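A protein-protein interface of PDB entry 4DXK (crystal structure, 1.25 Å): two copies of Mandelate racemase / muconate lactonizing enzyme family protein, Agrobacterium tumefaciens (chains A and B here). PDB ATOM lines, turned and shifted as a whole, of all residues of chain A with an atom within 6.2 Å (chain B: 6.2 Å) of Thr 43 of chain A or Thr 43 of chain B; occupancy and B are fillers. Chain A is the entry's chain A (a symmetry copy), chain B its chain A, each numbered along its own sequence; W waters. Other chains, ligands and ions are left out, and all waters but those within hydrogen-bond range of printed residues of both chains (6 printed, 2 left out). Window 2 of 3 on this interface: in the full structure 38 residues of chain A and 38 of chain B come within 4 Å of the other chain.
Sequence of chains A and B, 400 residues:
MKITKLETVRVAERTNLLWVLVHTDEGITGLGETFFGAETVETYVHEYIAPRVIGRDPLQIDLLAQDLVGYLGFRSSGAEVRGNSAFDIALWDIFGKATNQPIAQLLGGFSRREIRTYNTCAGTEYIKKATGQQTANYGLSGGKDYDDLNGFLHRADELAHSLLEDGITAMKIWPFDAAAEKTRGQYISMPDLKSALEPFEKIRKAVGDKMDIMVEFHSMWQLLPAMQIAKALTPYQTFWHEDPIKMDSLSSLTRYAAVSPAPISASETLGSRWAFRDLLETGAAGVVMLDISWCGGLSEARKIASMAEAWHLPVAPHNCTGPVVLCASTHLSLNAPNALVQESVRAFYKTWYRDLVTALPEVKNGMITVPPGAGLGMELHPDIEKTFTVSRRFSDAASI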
ATOM      1  N   ALA A  38     -20.656  23.884 -12.875  1.00  0.00           N
ATOM      2  CA  ALA A  38     -19.361  23.381 -12.440  1.00  0.00           C
ATOM      3  C   ALA A  38     -18.744  22.379 -13.415  1.00  0.00           C
ATOM      4  O   ALA A  38     -17.543  22.416 -13.651  1.00  0.00           O
ATOM      5  CB  ALA A  38     -19.472  22.775 -11.052  1.00  0.00           C
ATOM      6  N   GLU A  39     -19.544  21.480 -13.982  1.00  0.00           N
ATOM      7  CA  GLU A  39     -18.981  20.533 -14.946  1.00  0.00           C
ATOM      8  C   GLU A  39     -18.491  21.226 -16.217  1.00  0.00           C
ATOM      9  O   GLU A  39     -17.424  20.901 -16.753  1.00  0.00           O
ATOM     10  CB  GLU A  39     -19.988  19.447 -15.317  1.00  0.00           C
ATOM     11  CG  GLU A  39     -20.410  18.554 -14.167  1.00  0.00           C
ATOM     12  CD  GLU A  39     -21.500  17.572 -14.573  1.00  0.00           C
ATOM     13  OE1 GLU A  39     -21.926  17.603 -15.749  1.00  0.00           O
ATOM     14  OE2 GLU A  39     -21.934  16.781 -13.712  1.00  0.00           O
ATOM     15  N   THR A  40     -19.288  22.171 -16.702  1.00  0.00           N
ATOM     16  CA  THR A  40     -18.940  22.916 -17.902  1.00  0.00           C
ATOM     17  C   THR A  40     -17.654  23.718 -17.699  1.00  0.00           C
ATOM     18  O   THR A  40     -16.743  23.692 -18.536  1.00  0.00           O
ATOM     19  CB  THR A  40     -20.096  23.827 -18.322  1.00  0.00           C
ATOM     20  OG1 THR A  40     -21.220  23.003 -18.650  1.00  0.00           O
ATOM     21  CG2 THR A  40     -19.726  24.664 -19.535  1.00  0.00           C
ATOM     22  N   VAL A  41     -17.579  24.445 -16.593  1.00  0.00           N
ATOM     23  CA  VAL A  41     -16.396  25.236 -16.300  1.00  0.00           C
ATOM     24  C   VAL A  41     -15.175  24.333 -16.121  1.00  0.00           C
ATOM     25  O   VAL A  41     -14.090  24.641 -16.605  1.00  0.00           O
ATOM     26  CB  VAL A  41     -16.608  26.123 -15.065  1.00  0.00           C
ATOM     27  CG1 VAL A  41     -15.352  26.901 -14.756  1.00  0.00           C
ATOM     28  CG2 VAL A  41     -17.775  27.072 -15.304  1.00  0.00           C
ATOM     29  N   GLU A  42     -15.365  23.189 -15.478  1.00  0.00           N
ATOM     30  CA  GLU A  42     -14.275  22.233 -15.326  1.00  0.00           C
ATOM     31  C   GLU A  42     -13.727  21.792 -16.681  1.00  0.00           C
ATOM     32  O   GLU A  42     -12.509  21.742 -16.886  1.00  0.00           O
ATOM     33  CB  GLU A  42     -14.715  21.019 -14.518  1.00  0.00           C
ATOM     34  CG  GLU A  42     -13.672  19.904 -14.473  1.00  0.00           C
ATOM     35  CD  GLU A  42     -14.074  18.810 -13.530  1.00  0.00           C
ATOM     36  OE1 GLU A  42     -15.167  18.231 -13.718  1.00  0.00           O
ATOM     37  OE2 GLU A  42     -13.300  18.541 -12.591  1.00  0.00           O
ATOM     38  N   THR A  43     -14.620  21.460 -17.610  1.00  0.00           N
ATOM     39  CA  THR A  43     -14.170  21.051 -18.936  1.00  0.00           C
ATOM     40  C   THR A  43     -13.336  22.162 -19.571  1.00  0.00           C
ATOM     41  O   THR A  43     -12.292  21.912 -20.177  1.00  0.00           O
ATOM     42  CB  THR A  43     -15.356  20.699 -19.843  1.00  0.00           C
ATOM     43  OG1 THR A  43     -16.071  19.600 -19.271  1.00  0.00           O
ATOM     44  CG2 THR A  43     -14.878  20.304 -21.232  1.00  0.00           C
ATOM     45  N   TYR A  44     -13.803  23.397 -19.426  1.00  0.00           N
ATOM     46  CA  TYR A  44     -13.104  24.558 -19.966  1.00  0.00           C
ATOM     47  C   TYR A  44     -11.714  24.743 -19.352  1.00  0.00           C
ATOM     48  O   TYR A  44     -10.749  25.057 -20.057  1.00  0.00           O
ATOM     49  CB  TYR A  44     -13.948  25.820 -19.761  1.00  0.00           C
ATOM     50  CG  TYR A  44     -13.193  27.106 -20.023  1.00  0.00           C
ATOM     51  CD1 TYR A  44     -13.026  27.590 -21.317  1.00  0.00           C
ATOM     52  CD2 TYR A  44     -12.623  27.820 -18.983  1.00  0.00           C
ATOM     53  CE1 TYR A  44     -12.326  28.751 -21.557  1.00  0.00           C
ATOM     54  CE2 TYR A  44     -11.914  28.992 -19.214  1.00  0.00           C
ATOM     55  CZ  TYR A  44     -11.773  29.451 -20.509  1.00  0.00           C
ATOM     56  OH  TYR A  44     -11.095  30.619 -20.770  1.00  0.00           O
ATOM     57  N   VAL A  45     -11.608  24.569 -18.040  1.00  0.00           N
ATOM     58  CA  VAL A  45     -10.316  24.718 -17.379  1.00  0.00           C
ATOM     59  C   VAL A  45      -9.275  23.796 -18.012  1.00  0.00           C
ATOM     60  O   VAL A  45      -8.154  24.223 -18.288  1.00  0.00           O
ATOM     61  CB  VAL A  45     -10.438  24.465 -15.867  1.00  0.00           C
ATOM     62  CG1 VAL A  45      -9.076  24.378 -15.216  1.00  0.00           C
ATOM     63  CG2 VAL A  45     -11.264  25.566 -15.214  1.00  0.00           C
ATOM     64  N   HIS A  46      -9.663  22.554 -18.281  1.00  0.00           N
ATOM     65  CA  HIS A  46      -8.734  21.603 -18.876  1.00  0.00           C
ATOM     66  C   HIS A  46      -8.594  21.742 -20.392  1.00  0.00           C
ATOM     67  O   HIS A  46      -7.510  21.534 -20.924  1.00  0.00           O
ATOM     68  CB  HIS A  46      -9.099  20.178 -18.466  1.00  0.00           C
ATOM     69  CG  HIS A  46      -9.038  19.973 -16.991  1.00  0.00           C
ATOM     70  ND1 HIS A  46      -7.846  19.828 -16.313  1.00  0.00           N
ATOM     71  CD2 HIS A  46     -10.013  19.952 -16.052  1.00  0.00           C
ATOM     72  CE1 HIS A  46      -8.093  19.704 -15.020  1.00  0.00           C
ATOM     73  NE2 HIS A  46      -9.399  19.779 -14.836  1.00  0.00           N
ATOM     74  N   GLU A  47      -9.672  22.115 -21.082  1.00  0.00           N
ATOM     75  CA  GLU A  47      -9.641  22.237 -22.543  1.00  0.00           C
ATOM     76  C   GLU A  47      -8.875  23.484 -22.991  1.00  0.00           C
ATOM     77  O   GLU A  47      -8.122  23.441 -23.970  1.00  0.00           O
ATOM     78  CB  GLU A  47     -11.068  22.264 -23.127  1.00  0.00           C
ATOM     79  CG  GLU A  47     -11.127  22.327 -24.674  1.00  0.00           C
ATOM     80  CD  GLU A  47     -12.551  22.343 -25.258  1.00  0.00           C
ATOM     81  OE1 GLU A  47     -13.443  22.969 -24.654  1.00  0.00           O
ATOM     82  OE2 GLU A  47     -12.776  21.744 -26.336  1.00  0.00           O
ATOM     83  N   TYR A  48      -9.069  24.587 -22.274  1.00  0.00           N
ATOM     84  CA  TYR A  48      -8.617  25.908 -22.717  1.00  0.00           C
ATOM     85  C   TYR A  48      -7.517  26.511 -21.840  1.00  0.00           C
ATOM     86  O   TYR A  48      -6.489  26.961 -22.348  1.00  0.00           O
ATOM     87  CB  TYR A  48      -9.809  26.871 -22.778  1.00  0.00           C
ATOM     88  CG  TYR A  48      -9.506  28.159 -23.509  1.00  0.00           C
ATOM     89  CD1 TYR A  48      -8.987  29.270 -22.847  1.00  0.00           C
ATOM     90  CD2 TYR A  48      -9.731  28.257 -24.874  1.00  0.00           C
ATOM     91  CE1 TYR A  48      -8.702  30.439 -23.527  1.00  0.00           C
ATOM     92  CE2 TYR A  48      -9.454  29.419 -25.565  1.00  0.00           C
ATOM     93  CZ  TYR A  48      -8.944  30.505 -24.887  1.00  0.00           C
ATOM     94  OH  TYR A  48      -8.670  31.653 -25.598  1.00  0.00           O
ATOM     95  N   ARG A 393      -9.966  16.231 -11.341  1.00  0.00           N
ATOM     96  CA  ARG A 393      -9.357  16.056 -12.651  1.00  0.00           C
ATOM     97  C   ARG A 393      -8.093  16.898 -12.727  1.00  0.00           C
ATOM     98  O   ARG A 393      -8.038  18.007 -12.185  1.00  0.00           O
ATOM     99  CB  ARG A 393     -10.319  16.446 -13.766  1.00  0.00           C
ATOM    100  CG  ARG A 393      -9.746  16.183 -15.139  1.00  0.00           C
ATOM    101  CD  ARG A 393     -10.732  16.474 -16.249  1.00  0.00           C
ATOM    102  NE  ARG A 393     -10.046  16.456 -17.535  1.00  0.00           N
ATOM    103  CZ  ARG A 393     -10.560  16.923 -18.664  1.00  0.00           C
ATOM    104  NH1 ARG A 393     -11.775  17.460 -18.670  1.00  0.00           N
ATOM    105  NH2 ARG A 393      -9.852  16.866 -19.784  1.00  0.00           N
ATOM    106  N   ALA B  38     -15.459  22.917 -28.291  1.00  0.00           N
ATOM    107  CA  ALA B  38     -16.419  21.845 -28.515  1.00  0.00           C
ATOM    108  C   ALA B  38     -16.634  20.963 -27.286  1.00  0.00           C
ATOM    109  O   ALA B  38     -17.760  20.574 -27.003  1.00  0.00           O
ATOM    110  CB  ALA B  38     -15.999  21.005 -29.708  1.00  0.00           C
ATOM    111  N   GLU B  39     -15.572  20.635 -26.554  1.00  0.00           N
ATOM    112  CA  GLU B  39     -15.760  19.819 -25.353  1.00  0.00           C
ATOM    113  C   GLU B  39     -16.554  20.555 -24.273  1.00  0.00           C
ATOM    114  O   GLU B  39     -17.429  19.977 -23.616  1.00  0.00           O
ATOM    115  CB  GLU B  39     -14.423  19.360 -24.774  1.00  0.00           C
ATOM    116  CG  GLU B  39     -13.618  18.452 -25.682  1.00  0.00           C
ATOM    117  CD  GLU B  39     -12.250  18.127 -25.099  1.00  0.00           C
ATOM    118  OE1 GLU B  39     -11.936  18.622 -23.995  1.00  0.00           O
ATOM    119  OE2 GLU B  39     -11.490  17.387 -25.754  1.00  0.00           O
ATOM    120  N   THR B  40     -16.231  21.829 -24.087  1.00  0.00           N
ATOM    121  CA  THR B  40     -16.912  22.649 -23.098  1.00  0.00           C
ATOM    122  C   THR B  40     -18.398  22.788 -23.427  1.00  0.00           C
ATOM    123  O   THR B  40     -19.266  22.613 -22.563  1.00  0.00           O
ATOM    124  CB  THR B  40     -16.243  24.020 -22.985  1.00  0.00           C
ATOM    125  OG1 THR B  40     -14.902  23.829 -22.521  1.00  0.00           O
ATOM    126  CG2 THR B  40     -16.982  24.916 -22.005  1.00  0.00           C
ATOM    127  N   VAL B  41     -18.699  23.119 -24.676  1.00  0.00           N
ATOM    128  CA  VAL B  41     -20.082  23.267 -25.096  1.00  0.00           C
ATOM    129  C   VAL B  41     -20.827  21.938 -24.974  1.00  0.00           C
ATOM    130  O   VAL B  41     -21.969  21.896 -24.526  1.00  0.00           O
ATOM    131  CB  VAL B  41     -20.177  23.821 -26.524  1.00  0.00           C
ATOM    132  CG1 VAL B  41     -21.621  23.925 -26.952  1.00  0.00           C
ATOM    133  CG2 VAL B  41     -19.503  25.185 -26.597  1.00  0.00           C
ATOM    134  N   GLU B  42     -20.160  20.843 -25.316  1.00  0.00           N
ATOM    135  CA  GLU B  42     -20.766  19.527 -25.162  1.00  0.00           C
ATOM    136  C   GLU B  42     -21.163  19.262 -23.712  1.00  0.00           C
ATOM    137  O   GLU B  42     -22.269  18.781 -23.436  1.00  0.00           O
ATOM    138  CB  GLU B  42     -19.833  18.429 -25.659  1.00  0.00           C
ATOM    139  CG  GLU B  42     -20.338  17.019 -25.364  1.00  0.00           C
ATOM    140  CD  GLU B  42     -19.481  15.978 -26.020  1.00  0.00           C
ATOM    141  OE1 GLU B  42     -18.260  15.953 -25.751  1.00  0.00           O
ATOM    142  OE2 GLU B  42     -20.031  15.193 -26.817  1.00  0.00           O
ATOM    143  N   THR B  43     -20.263  19.562 -22.778  1.00  0.00           N
ATOM    144  CA  THR B  43     -20.583  19.357 -21.370  1.00  0.00           C
ATOM    145  C   THR B  43     -21.825  20.162 -20.993  1.00  0.00           C
ATOM    146  O   THR B  43     -22.712  19.677 -20.288  1.00  0.00           O
ATOM    147  CB  THR B  43     -19.406  19.751 -20.469  1.00  0.00           C
ATOM    148  OG1 THR B  43     -18.281  18.926 -20.782  1.00  0.00           O
ATOM    149  CG2 THR B  43     -19.760  19.564 -19.002  1.00  0.00           C
ATOM    150  N   TYR B  44     -21.885  21.400 -21.470  1.00  0.00           N
ATOM    151  CA  TYR B  44     -23.019  22.279 -21.205  1.00  0.00           C
ATOM    152  C   TYR B  44     -24.332  21.729 -21.771  1.00  0.00           C
ATOM    153  O   TYR B  44     -25.378  21.797 -21.116  1.00  0.00           O
ATOM    154  CB  TYR B  44     -22.742  23.677 -21.767  1.00  0.00           C
ATOM    155  CG  TYR B  44     -23.962  24.573 -21.799  1.00  0.00           C
ATOM    156  CD1 TYR B  44     -24.378  25.259 -20.663  1.00  0.00           C
ATOM    157  CD2 TYR B  44     -24.713  24.710 -22.954  1.00  0.00           C
ATOM    158  CE1 TYR B  44     -25.496  26.062 -20.688  1.00  0.00           C
ATOM    159  CE2 TYR B  44     -25.843  25.517 -22.989  1.00  0.00           C
ATOM    160  CZ  TYR B  44     -26.226  26.192 -21.847  1.00  0.00           C
ATOM    161  OH  TYR B  44     -27.328  27.014 -21.853  1.00  0.00           O
ATOM    162  N   VAL B  45     -24.288  21.202 -22.987  1.00  0.00           N
ATOM    163  CA  VAL B  45     -25.493  20.648 -23.594  1.00  0.00           C
ATOM    164  C   VAL B  45     -26.110  19.579 -22.694  1.00  0.00           C
ATOM    165  O   VAL B  45     -27.321  19.576 -22.474  1.00  0.00           O
ATOM    166  CB  VAL B  45     -25.198  20.091 -24.997  1.00  0.00           C
ATOM    167  CG1 VAL B  45     -26.374  19.304 -25.531  1.00  0.00           C
ATOM    168  CG2 VAL B  45     -24.849  21.227 -25.951  1.00  0.00           C
ATOM    169  N   HIS B  46     -25.272  18.709 -22.141  1.00  0.00           N
ATOM    170  CA  HIS B  46     -25.773  17.650 -21.275  1.00  0.00           C
ATOM    171  C   HIS B  46     -26.038  18.099 -19.838  1.00  0.00           C
ATOM    172  O   HIS B  46     -26.975  17.616 -19.213  1.00  0.00           O
ATOM    173  CB  HIS B  46     -24.845  16.438 -21.330  1.00  0.00           C
ATOM    174  CG  HIS B  46     -24.740  15.859 -22.700  1.00  0.00           C
ATOM    175  ND1 HIS B  46     -25.735  15.082 -23.254  1.00  0.00           N
ATOM    176  CD2 HIS B  46     -23.789  15.994 -23.654  1.00  0.00           C
ATOM    177  CE1 HIS B  46     -25.390  14.745 -24.484  1.00  0.00           C
ATOM    178  NE2 HIS B  46     -24.216  15.288 -24.751  1.00  0.00           N
ATOM    179  N   GLU B  47     -25.239  19.034 -19.324  1.00  0.00           N
ATOM    180  CA  GLU B  47     -25.395  19.499 -17.942  1.00  0.00           C
ATOM    181  C   GLU B  47     -26.619  20.404 -17.783  1.00  0.00           C
ATOM    182  O   GLU B  47     -27.343  20.312 -16.786  1.00  0.00           O
ATOM    183  CB  GLU B  47     -24.132  20.242 -17.461  1.00  0.00           C
ATOM    184  CG  GLU B  47     -24.187  20.713 -15.986  1.00  0.00           C
ATOM    185  CD  GLU B  47     -22.923  21.445 -15.502  1.00  0.00           C
ATOM    186  OE1 GLU B  47     -22.324  22.201 -16.293  1.00  0.00           O
ATOM    187  OE2 GLU B  47     -22.534  21.281 -14.322  1.00  0.00           O
ATOM    188  N   TYR B  48     -26.846  21.271 -18.765  1.00  0.00           N
ATOM    189  CA  TYR B  48     -27.812  22.366 -18.647  1.00  0.00           C
ATOM    190  C   TYR B  48     -29.012  22.233 -19.588  1.00  0.00           C
ATOM    191  O   TYR B  48     -30.160  22.347 -19.156  1.00  0.00           O
ATOM    192  CB  TYR B  48     -27.110  23.707 -18.896  1.00  0.00           C
ATOM    193  CG  TYR B  48     -27.943  24.904 -18.500  1.00  0.00           C
ATOM    194  CD1 TYR B  48     -28.828  25.507 -19.392  1.00  0.00           C
ATOM    195  CD2 TYR B  48     -27.850  25.426 -17.218  1.00  0.00           C
ATOM    196  CE1 TYR B  48     -29.593  26.595 -19.016  1.00  0.00           C
ATOM    197  CE2 TYR B  48     -28.607  26.513 -16.830  1.00  0.00           C
ATOM    198  CZ  TYR B  48     -29.472  27.094 -17.732  1.00  0.00           C
ATOM    199  OH  TYR B  48     -30.220  28.174 -17.321  1.00  0.00           O
ATOM    200  N   ARG B 393     -22.087  11.507 -27.261  1.00  0.00           N
ATOM    201  CA  ARG B 393     -22.645  11.439 -25.918  1.00  0.00           C
ATOM    202  C   ARG B 393     -24.142  11.694 -25.989  1.00  0.00           C
ATOM    203  O   ARG B 393     -24.607  12.512 -26.790  1.00  0.00           O
ATOM    204  CB  ARG B 393     -21.981  12.451 -24.992  1.00  0.00           C
ATOM    205  CG  ARG B 393     -22.474  12.337 -23.568  1.00  0.00           C
ATOM    206  CD  ARG B 393     -21.748  13.269 -22.622  1.00  0.00           C
ATOM    207  NE  ARG B 393     -22.439  13.304 -21.339  1.00  0.00           N
ATOM    208  CZ  ARG B 393     -22.216  14.206 -20.394  1.00  0.00           C
ATOM    209  NH1 ARG B 393     -21.320  15.168 -20.589  1.00  0.00           N
ATOM    210  NH2 ARG B 393     -22.901  14.156 -19.260  1.00  0.00           N
HETATM  211  O   HOH W   1     -11.633  19.199 -20.865  1.00  0.00           O
HETATM  212  O   HOH W   2     -12.763  22.770 -29.349  1.00  0.00           O
HETATM  213  O   HOH W   3     -22.265  17.198 -18.901  1.00  0.00           O
HETATM  214  O   HOH W   4     -11.041  19.962 -27.480  1.00  0.00           O
HETATM  215  O   HOH W   5     -23.469  19.306 -12.673  1.00  0.00           O
HETATM  216  O   HOH W   6     -23.120  22.942 -11.671  1.00  0.00           O
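Hydrophobic or aromatic side chains of chain A within 4 Å of the printed part of chain B: Tyr 44. Hydrophobic or aromatic side chains of chain B that line the printed part of chain A: Tyr 44. Among the printed residues, 14 pairs touch across the chains.
Water W5 bridges the side-chain carboxylate (OE2) of Glu 47 of chain B and the side-chain carboxylate (OE2) of Glu 39 of chain A. Water W4 lies within hydrogen-bond range of the side-chain carboxylate (OE2) of Glu 47 of chain A (2.7 Å) and the side-chain carboxylate (OE2) of Glu 39 of chain B (3.1 Å). Water W3 lies within hydrogen-bond range of NH1 of Arg 393 of chain B (2.8 Å), O of Thr 43 of chain B (2.9 Å) and OE1 of Glu 39 of chain A (3.2 Å). Water W1 lies within hydrogen-bond range of the guanidinium group (NH1) of Arg 393 of chain A (2.8 Å), the backbone carbonyl oxygen (O) of Thr 43 of chain A (2.9 Å) and the side-chain carboxylate (OE1) of Glu 39 of chain B (3.2 Å). Water W2 bridges the backbone NH (N) of Ala 38 of chain B (2.9 Å) and the side-chain carboxylate (OE2) of Glu 47 of chain A (3.2 Å). Water W6 lies within hydrogen-bond range of the backbone NH (N) of Ala 38 of chain A (2.9 Å) and the side-chain carboxylate (OE2) of Glu 47 of chain B (3.2 Å).
Glu 39 of chain A touches Thr 43 of chain B, and with the chains exchanged Thr 43 of chain A touches Glu 39 of chain B. Glu 39 of chain A touches Glu 47 of chain B, and with the chains exchanged Glu 47 of chain A touches Glu 39 of chain B. Thr 40 of chain A touches Glu 47 of chain B, and with the chains exchanged Glu 47 of chain A touches Thr 40 of chain B. Thr 43 of chain A touches its own counterpart, Thr 43 of chain B. Positions printed for both chains: 38, 39, 40, 41, 42, 43, 44, 45, 46, 47, 48 and 393.
Among the printed residues, merely in contact across the chains: Thr 43 of chain A with Glu 39 of chain B (3.5 Å), Glu 39 of chain A with Thr 43 of chain B (3.5 Å), Thr 43 of chain A with Thr 40 of chain B (3.5 Å), Thr 40 of chain A with Thr 43 of chain B (3.5 Å), Ala 38 of chain A with Glu 47 of chain B (3.5 Å), Glu 47 of chain A with Ala 38 of chain B (3.5 Å) and Thr 40 of chain A with Thr 40 of chain B (3.7 Å).
OG1 of Thr 43 of chain B is in hydrogen-bond range of O of Glu 39 of chain B (3.1 Å). The backbone carbonyl oxygen (O) of Glu 39 of chain A lies within hydrogen-bond range of the side-chain hydroxyl (OG1) of Thr 43 of chain A (3.1 Å).
Of the printed residues of chain B, Ala 38 of chain A touches Glu 47. Printed residues of chain B within 4 Å of Glu 39 of chain A: Thr 43 and Glu 47. Thr 43 of chain A touches just these residues of chain B: Glu 39, Thr 40 and Thr 43. Of the printed residues of chain B, Tyr 44 of chain A touches Thr 40. Of the printed residues of chain B, Glu 47 of chain A touches Ala 38 (3.5 Å), Glu 39 (3.0 Å) and Thr 40 (2.7 Å). Tyr 48 of chain A touches none of the printed residues of chain B. Thr 43 of chain B touches three residues of chain A. Of the printed residues of chain A, Glu 47 of chain B touches Ala 38, Glu 39 and Thr 40. The nearest residue of chain B that does not touch Thr 43 of chain A is Val 41 of chain B (5.9 Å).
The side-chain carboxylate of Glu 47 of chain B sits at hydrogen-bond distance from the side-chain hydroxyl of Thr 40 of chain A. The backbone NH (N) of Glu 39 of chain A lies within hydrogen-bond range of the side-chain carboxylate (OE2) of Glu 47 of chain B. The backbone NH of Glu 39 of chain B sits at hydrogen-bond distance from the side-chain carboxylate of Glu 47 of chain A. OG1 of Thr 43 of chain B sits at hydrogen-bond distance from OG1 of Thr 43 of chain A, 2.8 Å away. The side-chain hydroxyl (OG1) of Thr 40 of chain A lies close to the backbone NH (N) of Tyr 44 of chain B (3.3 Å). OG1 of Thr 40 of chain B sits at hydrogen-bond distance from OE1 of Glu 47 of chain A (2.7 Å). The side-chain hydroxyl of Thr 40 of chain B lies close to the backbone NH of Tyr 44 of chain A, 3.3 Å away.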
